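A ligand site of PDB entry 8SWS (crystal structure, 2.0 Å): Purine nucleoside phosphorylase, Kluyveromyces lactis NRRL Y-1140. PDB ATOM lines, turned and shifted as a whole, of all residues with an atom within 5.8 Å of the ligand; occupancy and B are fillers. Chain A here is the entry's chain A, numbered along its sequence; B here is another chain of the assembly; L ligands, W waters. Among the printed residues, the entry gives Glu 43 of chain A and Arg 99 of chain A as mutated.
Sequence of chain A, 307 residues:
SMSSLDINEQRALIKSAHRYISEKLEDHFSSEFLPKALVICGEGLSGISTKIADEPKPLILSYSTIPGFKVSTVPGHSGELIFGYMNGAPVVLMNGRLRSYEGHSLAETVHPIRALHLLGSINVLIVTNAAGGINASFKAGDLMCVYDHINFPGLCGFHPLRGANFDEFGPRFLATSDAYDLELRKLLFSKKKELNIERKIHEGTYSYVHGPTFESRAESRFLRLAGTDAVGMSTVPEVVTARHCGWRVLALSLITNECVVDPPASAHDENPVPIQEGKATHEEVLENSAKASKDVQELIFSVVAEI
OE1 of Glu 215 is in hydrogen-bond range of N2 of the ligand, 2.6 Å away. O3 of the ligand sits at hydrogen-bond distance from ND1 of His 282 (2.6 Å). The side-chain amide nitrogen of Asn 257 is in hydrogen-bond range of an oxygen (O1) of the ligand (2.8 Å). An oxygen (O2) of the ligand is in hydrogen-bond range of the side-chain hydroxyl (OH) of Tyr 101 (2.9 Å). N of Gly 132 sits close to N4 of the ligand (3.4 Å).
OD1 of Asn 257 sits at hydrogen-bond distance from OG1 of Thr 256. O of Asn 257 sits at hydrogen-bond distance from N of Gly 133, at 2.7 Å. The side-chain hydroxyl of Tyr 101 is in hydrogen-bond range of the guanidinium group of Arg 99. N of Gly 132 is in hydrogen-bond range of O of Val 231 (2.8 Å). OH of Tyr 206 sits at hydrogen-bond distance from N of Met 233 (3.3 Å). The backbone carbonyl oxygen (O) of Gly 232 is in hydrogen-bond range of the backbone NH (N) of Val 209 (2.9 Å). N of Thr 256 is in hydrogen-bond range of O of Ala 131, at 2.9 Å.
Merely in contact with the ligand: Glu 43 (3.998 Å), Arg 99 (3.9 Å), Ala 130 (3.0 Å), Ala 131 (3.6 Å), Val 209 (3.7 Å), Phe 214 (3.5 Å), Val 231 (3.5 Å), Gly 232 (3.4 Å), Met 233 (3.4 Å), Thr 256 (3.5 Å), Val 285 (3.5 Å) and Phe 173 of chain B (3.5 Å). Hydrophobic or aromatic side chains within 4 Å of the ligand: Tyr 101, Val 209, Phe 214, Val 231, Met 233, His 282, Val 285 and Phe 173 of chain B. Within 4 Å of the ligand: Glu 43, Arg 99, Tyr 101, Ala 130, Ala 131, Gly 132, Val 209, Phe 214, Glu 215, Val 231, Gly 232, Met 233, Thr 256, Asn 257, His 282, Val 285 and Phe 173 of chain B. Along chain A the residues within 4 Å of the ligand span positions 43 to 285.
Water W2 lies within hydrogen-bond range of the side-chain carboxylate (OE2) of Glu 215, an oxygen (O1) of the ligand and the side-chain sulfur (SG) of Cys 259. Water W1 lies within hydrogen-bond range of O of Ala 130, OH of Tyr 206 and N of Met 233.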
ATOM      1  N   GLU A  43       7.188  19.042   5.733  1.00  0.00           N
ATOM      2  CA  GLU A  43       7.615  18.704   7.086  1.00  0.00           C
ATOM      3  C   GLU A  43       7.399  19.843   8.066  1.00  0.00           C
ATOM      4  O   GLU A  43       7.939  20.940   7.876  1.00  0.00           O
ATOM      5  CB  GLU A  43       9.091  18.304   7.064  1.00  0.00           C
ATOM      6  CG  GLU A  43       9.296  16.832   7.025  1.00  0.00           C
ATOM      7  CD  GLU A  43       9.331  16.254   8.421  1.00  0.00           C
ATOM      8  OE1 GLU A  43       8.254  16.225   9.063  1.00  0.00           O
ATOM      9  OE2 GLU A  43      10.419  15.827   8.867  1.00  0.00           O
ATOM     10  N   ARG A  99       7.913   9.776   0.925  1.00  0.00           N
ATOM     11  CA  ARG A  99       9.203  10.182   0.395  1.00  0.00           C
ATOM     12  C   ARG A  99       9.997   8.931  -0.019  1.00  0.00           C
ATOM     13  O   ARG A  99       9.874   7.862   0.599  1.00  0.00           O
ATOM     14  CB  ARG A  99       9.965  11.052   1.403  1.00  0.00           C
ATOM     15  CG  ARG A  99       9.640  12.560   1.252  1.00  0.00           C
ATOM     16  CD  ARG A  99       9.813  13.320   2.586  1.00  0.00           C
ATOM     17  NE  ARG A  99       9.064  12.662   3.649  1.00  0.00           N
ATOM     18  CZ  ARG A  99       8.371  13.281   4.603  1.00  0.00           C
ATOM     19  NH1 ARG A  99       8.266  14.606   4.650  1.00  0.00           N
ATOM     20  NH2 ARG A  99       7.754  12.550   5.526  1.00  0.00           N
ATOM     21  N   TYR A 101      13.108   7.911  -0.023  1.00  0.00           N
ATOM     22  CA  TYR A 101      14.089   7.283   0.870  1.00  0.00           C
ATOM     23  C   TYR A 101      13.483   6.300   1.862  1.00  0.00           C
ATOM     24  O   TYR A 101      14.237   5.587   2.542  1.00  0.00           O
ATOM     25  CB  TYR A 101      14.903   8.311   1.659  1.00  0.00           C
ATOM     26  CG  TYR A 101      14.091   9.222   2.560  1.00  0.00           C
ATOM     27  CD1 TYR A 101      13.524   8.758   3.756  1.00  0.00           C
ATOM     28  CD2 TYR A 101      13.948  10.554   2.233  1.00  0.00           C
ATOM     29  CE1 TYR A 101      12.784   9.617   4.574  1.00  0.00           C
ATOM     30  CE2 TYR A 101      13.240  11.412   3.052  1.00  0.00           C
ATOM     31  CZ  TYR A 101      12.660  10.950   4.208  1.00  0.00           C
ATOM     32  OH  TYR A 101      11.970  11.843   4.965  1.00  0.00           O
ATOM     33  N   ALA A 130      10.274  21.809   3.514  1.00  0.00           N
ATOM     34  CA  ALA A 130      11.439  22.337   4.209  1.00  0.00           C
ATOM     35  C   ALA A 130      12.678  22.048   3.370  1.00  0.00           C
ATOM     36  O   ALA A 130      12.719  21.057   2.648  1.00  0.00           O
ATOM     37  CB  ALA A 130      11.565  21.681   5.594  1.00  0.00           C
ATOM     38  N   ALA A 131      13.689  22.907   3.463  1.00  0.00           N
ATOM     39  CA  ALA A 131      14.858  22.733   2.602  1.00  0.00           C
ATOM     40  C   ALA A 131      16.107  23.289   3.273  1.00  0.00           C
ATOM     41  O   ALA A 131      16.036  24.218   4.084  1.00  0.00           O
ATOM     42  CB  ALA A 131      14.653  23.405   1.227  1.00  0.00           C
ATOM     43  N   GLY A 132      17.256  22.718   2.916  1.00  0.00           N
ATOM     44  CA  GLY A 132      18.545  23.290   3.319  1.00  0.00           C
ATOM     45  C   GLY A 132      18.954  24.438   2.397  1.00  0.00           C
ATOM     46  O   GLY A 132      18.763  24.388   1.166  1.00  0.00           O
ATOM     47  N   GLY A 133      19.519  25.485   2.987  1.00  0.00           N
ATOM     48  CA  GLY A 133      19.933  26.635   2.176  1.00  0.00           C
ATOM     49  C   GLY A 133      21.297  26.420   1.546  1.00  0.00           C
ATOM     50  O   GLY A 133      22.281  26.234   2.272  1.00  0.00           O
ATOM     51  N   TYR A 206      15.113  24.908  -6.625  1.00  0.00           N
ATOM     52  CA  TYR A 206      15.062  23.782  -5.690  1.00  0.00           C
ATOM     53  C   TYR A 206      15.632  22.530  -6.347  1.00  0.00           C
ATOM     54  O   TYR A 206      15.232  22.185  -7.467  1.00  0.00           O
ATOM     55  CB  TYR A 206      13.613  23.542  -5.248  1.00  0.00           C
ATOM     56  CG  TYR A 206      13.417  22.361  -4.317  1.00  0.00           C
ATOM     57  CD1 TYR A 206      13.201  21.065  -4.843  1.00  0.00           C
ATOM     58  CD2 TYR A 206      13.433  22.515  -2.920  1.00  0.00           C
ATOM     59  CE1 TYR A 206      13.001  19.969  -4.011  1.00  0.00           C
ATOM     60  CE2 TYR A 206      13.229  21.413  -2.067  1.00  0.00           C
ATOM     61  CZ  TYR A 206      13.017  20.129  -2.621  1.00  0.00           C
ATOM     62  OH  TYR A 206      12.799  19.043  -1.808  1.00  0.00           O
ATOM     63  N   VAL A 209      17.145  15.685  -3.983  1.00  0.00           N
ATOM     64  CA  VAL A 209      18.064  14.557  -3.831  1.00  0.00           C
ATOM     65  C   VAL A 209      17.365  13.471  -3.018  1.00  0.00           C
ATOM     66  O   VAL A 209      16.389  13.734  -2.296  1.00  0.00           O
ATOM     67  CB  VAL A 209      19.406  14.985  -3.177  1.00  0.00           C
ATOM     68  CG1 VAL A 209      20.073  16.123  -3.985  1.00  0.00           C
ATOM     69  CG2 VAL A 209      19.196  15.405  -1.713  1.00  0.00           C
ATOM     70  N   GLY A 211      18.256  11.498  -0.406  1.00  0.00           N
ATOM     71  CA  GLY A 211      18.380  11.385   1.025  1.00  0.00           C
ATOM     72  C   GLY A 211      18.644   9.936   1.429  1.00  0.00           C
ATOM     73  O   GLY A 211      18.903   9.080   0.559  1.00  0.00           O
ATOM     74  N   THR A 213      20.515  10.927   4.151  1.00  0.00           N
ATOM     75  CA  THR A 213      21.600  11.718   4.701  1.00  0.00           C
ATOM     76  C   THR A 213      21.441  13.198   4.358  1.00  0.00           C
ATOM     77  O   THR A 213      20.926  13.572   3.303  1.00  0.00           O
ATOM     78  CB  THR A 213      22.912  11.244   4.103  1.00  0.00           C
ATOM     79  OG1 THR A 213      22.719  11.044   2.695  1.00  0.00           O
ATOM     80  CG2 THR A 213      23.346   9.933   4.777  1.00  0.00           C
ATOM     81  N   PHE A 214      21.823  14.052   5.304  1.00  0.00           N
ATOM     82  CA  PHE A 214      22.091  15.442   4.958  1.00  0.00           C
ATOM     83  C   PHE A 214      23.405  15.546   4.182  1.00  0.00           C
ATOM     84  O   PHE A 214      24.300  14.702   4.332  1.00  0.00           O
ATOM     85  CB  PHE A 214      22.131  16.318   6.227  1.00  0.00           C
ATOM     86  CG  PHE A 214      20.806  16.425   6.965  1.00  0.00           C
ATOM     87  CD1 PHE A 214      19.740  17.165   6.427  1.00  0.00           C
ATOM     88  CD2 PHE A 214      20.633  15.836   8.231  1.00  0.00           C
ATOM     89  CE1 PHE A 214      18.505  17.286   7.127  1.00  0.00           C
ATOM     90  CE2 PHE A 214      19.414  15.967   8.943  1.00  0.00           C
ATOM     91  CZ  PHE A 214      18.354  16.687   8.399  1.00  0.00           C
ATOM     92  N   GLU A 215      23.544  16.627   3.400  1.00  0.00           N
ATOM     93  CA  GLU A 215      24.596  16.688   2.394  1.00  0.00           C
ATOM     94  C   GLU A 215      25.966  16.804   3.051  1.00  0.00           C
ATOM     95  O   GLU A 215      26.128  17.493   4.050  1.00  0.00           O
ATOM     96  CB  GLU A 215      24.418  17.927   1.494  1.00  0.00           C
ATOM     97  CG  GLU A 215      23.290  17.691   0.486  1.00  0.00           C
ATOM     98  CD  GLU A 215      21.922  17.629   1.190  1.00  0.00           C
ATOM     99  OE1 GLU A 215      20.989  17.014   0.605  1.00  0.00           O
ATOM    100  OE2 GLU A 215      21.763  18.317   2.264  1.00  0.00           O
ATOM    101  N   VAL A 231      17.896  22.802  -1.147  1.00  0.00           N
ATOM    102  CA  VAL A 231      17.952  21.364  -1.421  1.00  0.00           C
ATOM    103  C   VAL A 231      17.023  20.630  -0.464  1.00  0.00           C
ATOM    104  O   VAL A 231      17.009  20.894   0.747  1.00  0.00           O
ATOM    105  CB  VAL A 231      19.383  20.799  -1.338  1.00  0.00           C
ATOM    106  CG1 VAL A 231      20.011  21.016   0.030  1.00  0.00           C
ATOM    107  CG2 VAL A 231      19.404  19.238  -1.630  1.00  0.00           C
ATOM    108  N   GLY A 232      16.239  19.698  -1.017  1.00  0.00           N
ATOM    109  CA  GLY A 232      15.365  18.869  -0.211  1.00  0.00           C
ATOM    110  C   GLY A 232      15.216  17.467  -0.761  1.00  0.00           C
ATOM    111  O   GLY A 232      15.883  17.095  -1.722  1.00  0.00           O
ATOM    112  N   MET A 233      14.334  16.663  -0.162  1.00  0.00           N
ATOM    113  CA  MET A 233      14.214  15.247  -0.508  1.00  0.00           C
ATOM    114  C   MET A 233      12.834  14.916  -1.036  1.00  0.00           C
ATOM    115  O   MET A 233      12.373  13.802  -0.856  1.00  0.00           O
ATOM    116  CB  MET A 233      14.507  14.400   0.727  1.00  0.00           C
ATOM    117  CG  MET A 233      15.871  14.611   1.335  1.00  0.00           C
ATOM    118  SD  MET A 233      16.065  13.631   2.835  1.00  0.00           S
ATOM    119  CE  MET A 233      17.602  14.291   3.441  1.00  0.00           C
ATOM    120  N   THR A 256      15.070  25.750   6.404  1.00  0.00           N
ATOM    121  CA  THR A 256      15.145  25.338   7.805  1.00  0.00           C
ATOM    122  C   THR A 256      16.550  25.287   8.366  1.00  0.00           C
ATOM    123  O   THR A 256      16.700  25.141   9.580  1.00  0.00           O
ATOM    124  CB  THR A 256      14.504  23.969   7.986  1.00  0.00           C
ATOM    125  OG1 THR A 256      15.101  23.081   7.040  1.00  0.00           O
ATOM    126  CG2 THR A 256      12.995  24.068   7.733  1.00  0.00           C
ATOM    127  N   ASN A 257      17.566  25.440   7.523  1.00  0.00           N
ATOM    128  CA  ASN A 257      18.962  25.283   7.948  1.00  0.00           C
ATOM    129  C   ASN A 257      19.848  25.728   6.794  1.00  0.00           C
ATOM    130  O   ASN A 257      19.431  25.679   5.631  1.00  0.00           O
ATOM    131  CB  ASN A 257      19.267  23.835   8.354  1.00  0.00           C
ATOM    132  CG  ASN A 257      18.927  22.840   7.256  1.00  0.00           C
ATOM    133  OD1 ASN A 257      17.756  22.614   6.957  1.00  0.00           O
ATOM    134  ND2 ASN A 257      19.955  22.235   6.645  1.00  0.00           N
ATOM    135  N   CYS A 259      23.125  24.920   4.668  1.00  0.00           N
ATOM    136  CA  CYS A 259      23.970  23.769   4.402  1.00  0.00           C
ATOM    137  C   CYS A 259      25.446  24.109   4.647  1.00  0.00           C
ATOM    138  O   CYS A 259      25.895  25.238   4.413  1.00  0.00           O
ATOM    139  CB  CYS A 259      23.785  23.264   2.947  1.00  0.00           C
ATOM    140  SG  CYS A 259      22.057  22.888   2.561  1.00  0.00           S
ATOM    141  N   ALA A 280      23.689  19.682  10.287  1.00  0.00           N
ATOM    142  CA  ALA A 280      22.228  19.568  10.234  1.00  0.00           C
ATOM    143  C   ALA A 280      21.732  18.503  11.227  1.00  0.00           C
ATOM    144  O   ALA A 280      22.409  17.490  11.469  1.00  0.00           O
ATOM    145  CB  ALA A 280      21.790  19.206   8.800  1.00  0.00           C
ATOM    146  N   THR A 281      20.558  18.750  11.829  1.00  0.00           N
ATOM    147  CA  THR A 281      19.821  17.741  12.601  1.00  0.00           C
ATOM    148  C   THR A 281      18.344  17.792  12.211  1.00  0.00           C
ATOM    149  O   THR A 281      17.830  18.834  11.790  1.00  0.00           O
ATOM    150  CB  THR A 281      19.885  17.927  14.125  1.00  0.00           C
ATOM    151  OG1 THR A 281      19.350  19.212  14.476  1.00  0.00           O
ATOM    152  CG2 THR A 281      21.315  17.798  14.644  1.00  0.00           C
ATOM    153  N   HIS A 282      17.648  16.668  12.422  1.00  0.00           N
ATOM    154  CA  HIS A 282      16.197  16.650  12.201  1.00  0.00           C
ATOM    155  C   HIS A 282      15.501  17.654  13.113  1.00  0.00           C
ATOM    156  O   HIS A 282      14.608  18.398  12.682  1.00  0.00           O
ATOM    157  CB  HIS A 282      15.629  15.259  12.488  1.00  0.00           C
ATOM    158  CG  HIS A 282      14.209  15.093  12.040  1.00  0.00           C
ATOM    159  ND1 HIS A 282      13.708  15.755  10.950  1.00  0.00           N
ATOM    160  CD2 HIS A 282      13.206  14.315  12.506  1.00  0.00           C
ATOM    161  CE1 HIS A 282      12.450  15.414  10.757  1.00  0.00           C
ATOM    162  NE2 HIS A 282      12.104  14.553  11.700  1.00  0.00           N
ATOM    163  N   VAL A 285      15.479  21.147  11.928  1.00  0.00           N
ATOM    164  CA  VAL A 285      14.565  21.300  10.798  1.00  0.00           C
ATOM    165  C   VAL A 285      13.146  21.453  11.315  1.00  0.00           C
ATOM    166  O   VAL A 285      12.397  22.343  10.863  1.00  0.00           O
ATOM    167  CB  VAL A 285      14.673  20.107   9.830  1.00  0.00           C
ATOM    168  CG1 VAL A 285      13.583  20.169   8.770  1.00  0.00           C
ATOM    169  CG2 VAL A 285      16.045  20.063   9.153  1.00  0.00           C
ATOM    170  N   LEU A 286      12.746  20.573  12.237  1.00  0.00           N
ATOM    171  CA  LEU A 286      11.401  20.614  12.805  1.00  0.00           C
ATOM    172  C   LEU A 286      11.137  21.920  13.542  1.00  0.00           C
ATOM    173  O   LEU A 286      10.024  22.456  13.465  1.00  0.00           O
ATOM    174  CB  LEU A 286      11.160  19.443  13.783  1.00  0.00           C
ATOM    175  CG  LEU A 286      11.191  18.037  13.145  1.00  0.00           C
ATOM    176  CD1 LEU A 286      11.324  16.913  14.227  1.00  0.00           C
ATOM    177  CD2 LEU A 286      10.019  17.825  12.169  1.00  0.00           C
ATOM    178  N   PHE B 173      17.922  10.689   9.921  1.00  0.00           N
ATOM    179  CA  PHE B 173      18.563  11.660   9.054  1.00  0.00           C
ATOM    180  C   PHE B 173      19.959  11.944   9.595  1.00  0.00           C
ATOM    181  O   PHE B 173      20.128  12.703  10.550  1.00  0.00           O
ATOM    182  CB  PHE B 173      17.711  12.932   8.943  1.00  0.00           C
ATOM    183  CG  PHE B 173      16.274  12.643   8.531  1.00  0.00           C
ATOM    184  CD1 PHE B 173      15.975  12.351   7.209  1.00  0.00           C
ATOM    185  CD2 PHE B 173      15.228  12.750   9.460  1.00  0.00           C
ATOM    186  CE1 PHE B 173      14.652  12.119   6.801  1.00  0.00           C
ATOM    187  CE2 PHE B 173      13.914  12.507   9.069  1.00  0.00           C
ATOM    188  CZ  PHE B 173      13.626  12.186   7.721  1.00  0.00           C
HETATM  189  N1  LIG L   1      19.024  18.690   3.093  1.00  0.00           N
HETATM  190  C1  LIG L   1      18.097  17.919   2.435  1.00  0.00           C
HETATM  191  N2  LIG L   1      18.571  17.087   1.479  1.00  0.00           N
HETATM  192  N3  LIG L   1      16.813  17.971   2.733  1.00  0.00           N
HETATM  193  C2  LIG L   1      16.426  18.843   3.731  1.00  0.00           C
HETATM  194  C3  LIG L   1      17.339  19.657   4.414  1.00  0.00           C
HETATM  195  C4  LIG L   1      18.721  19.606   4.096  1.00  0.00           C
HETATM  196  O1  LIG L   1      19.617  20.282   4.611  1.00  0.00           O
HETATM  197  N4  LIG L   1      16.634  20.399   5.317  1.00  0.00           N
HETATM  198  C5  LIG L   1      15.318  20.070   5.227  1.00  0.00           C
HETATM  199  C6  LIG L   1      15.159  19.118   4.259  1.00  0.00           C
HETATM  200  N5  LIG L   1      13.472  17.289   4.558  1.00  0.00           N
HETATM  201  C7  LIG L   1      13.845  18.527   3.850  1.00  0.00           C
HETATM  202  C8  LIG L   1      14.435  16.193   4.363  1.00  0.00           C
HETATM  203  C9  LIG L   1      13.898  15.169   5.322  1.00  0.00           C
HETATM  204  O2  LIG L   1      12.672  14.673   4.815  1.00  0.00           O
HETATM  205  C10 LIG L   1      13.700  16.031   6.592  1.00  0.00           C
HETATM  206  C11 LIG L   1      14.933  16.117   7.456  1.00  0.00           C
HETATM  207  O3  LIG L   1      14.661  16.747   8.702  1.00  0.00           O
HETATM  208  C12 LIG L   1      13.350  17.417   6.031  1.00  0.00           C
HETATM  209  O   HOH W   1      12.290  19.235   0.850  1.00  0.00           O
HETATM  210  O   HOH W   2      22.592  19.762   4.499  1.00  0.00           O
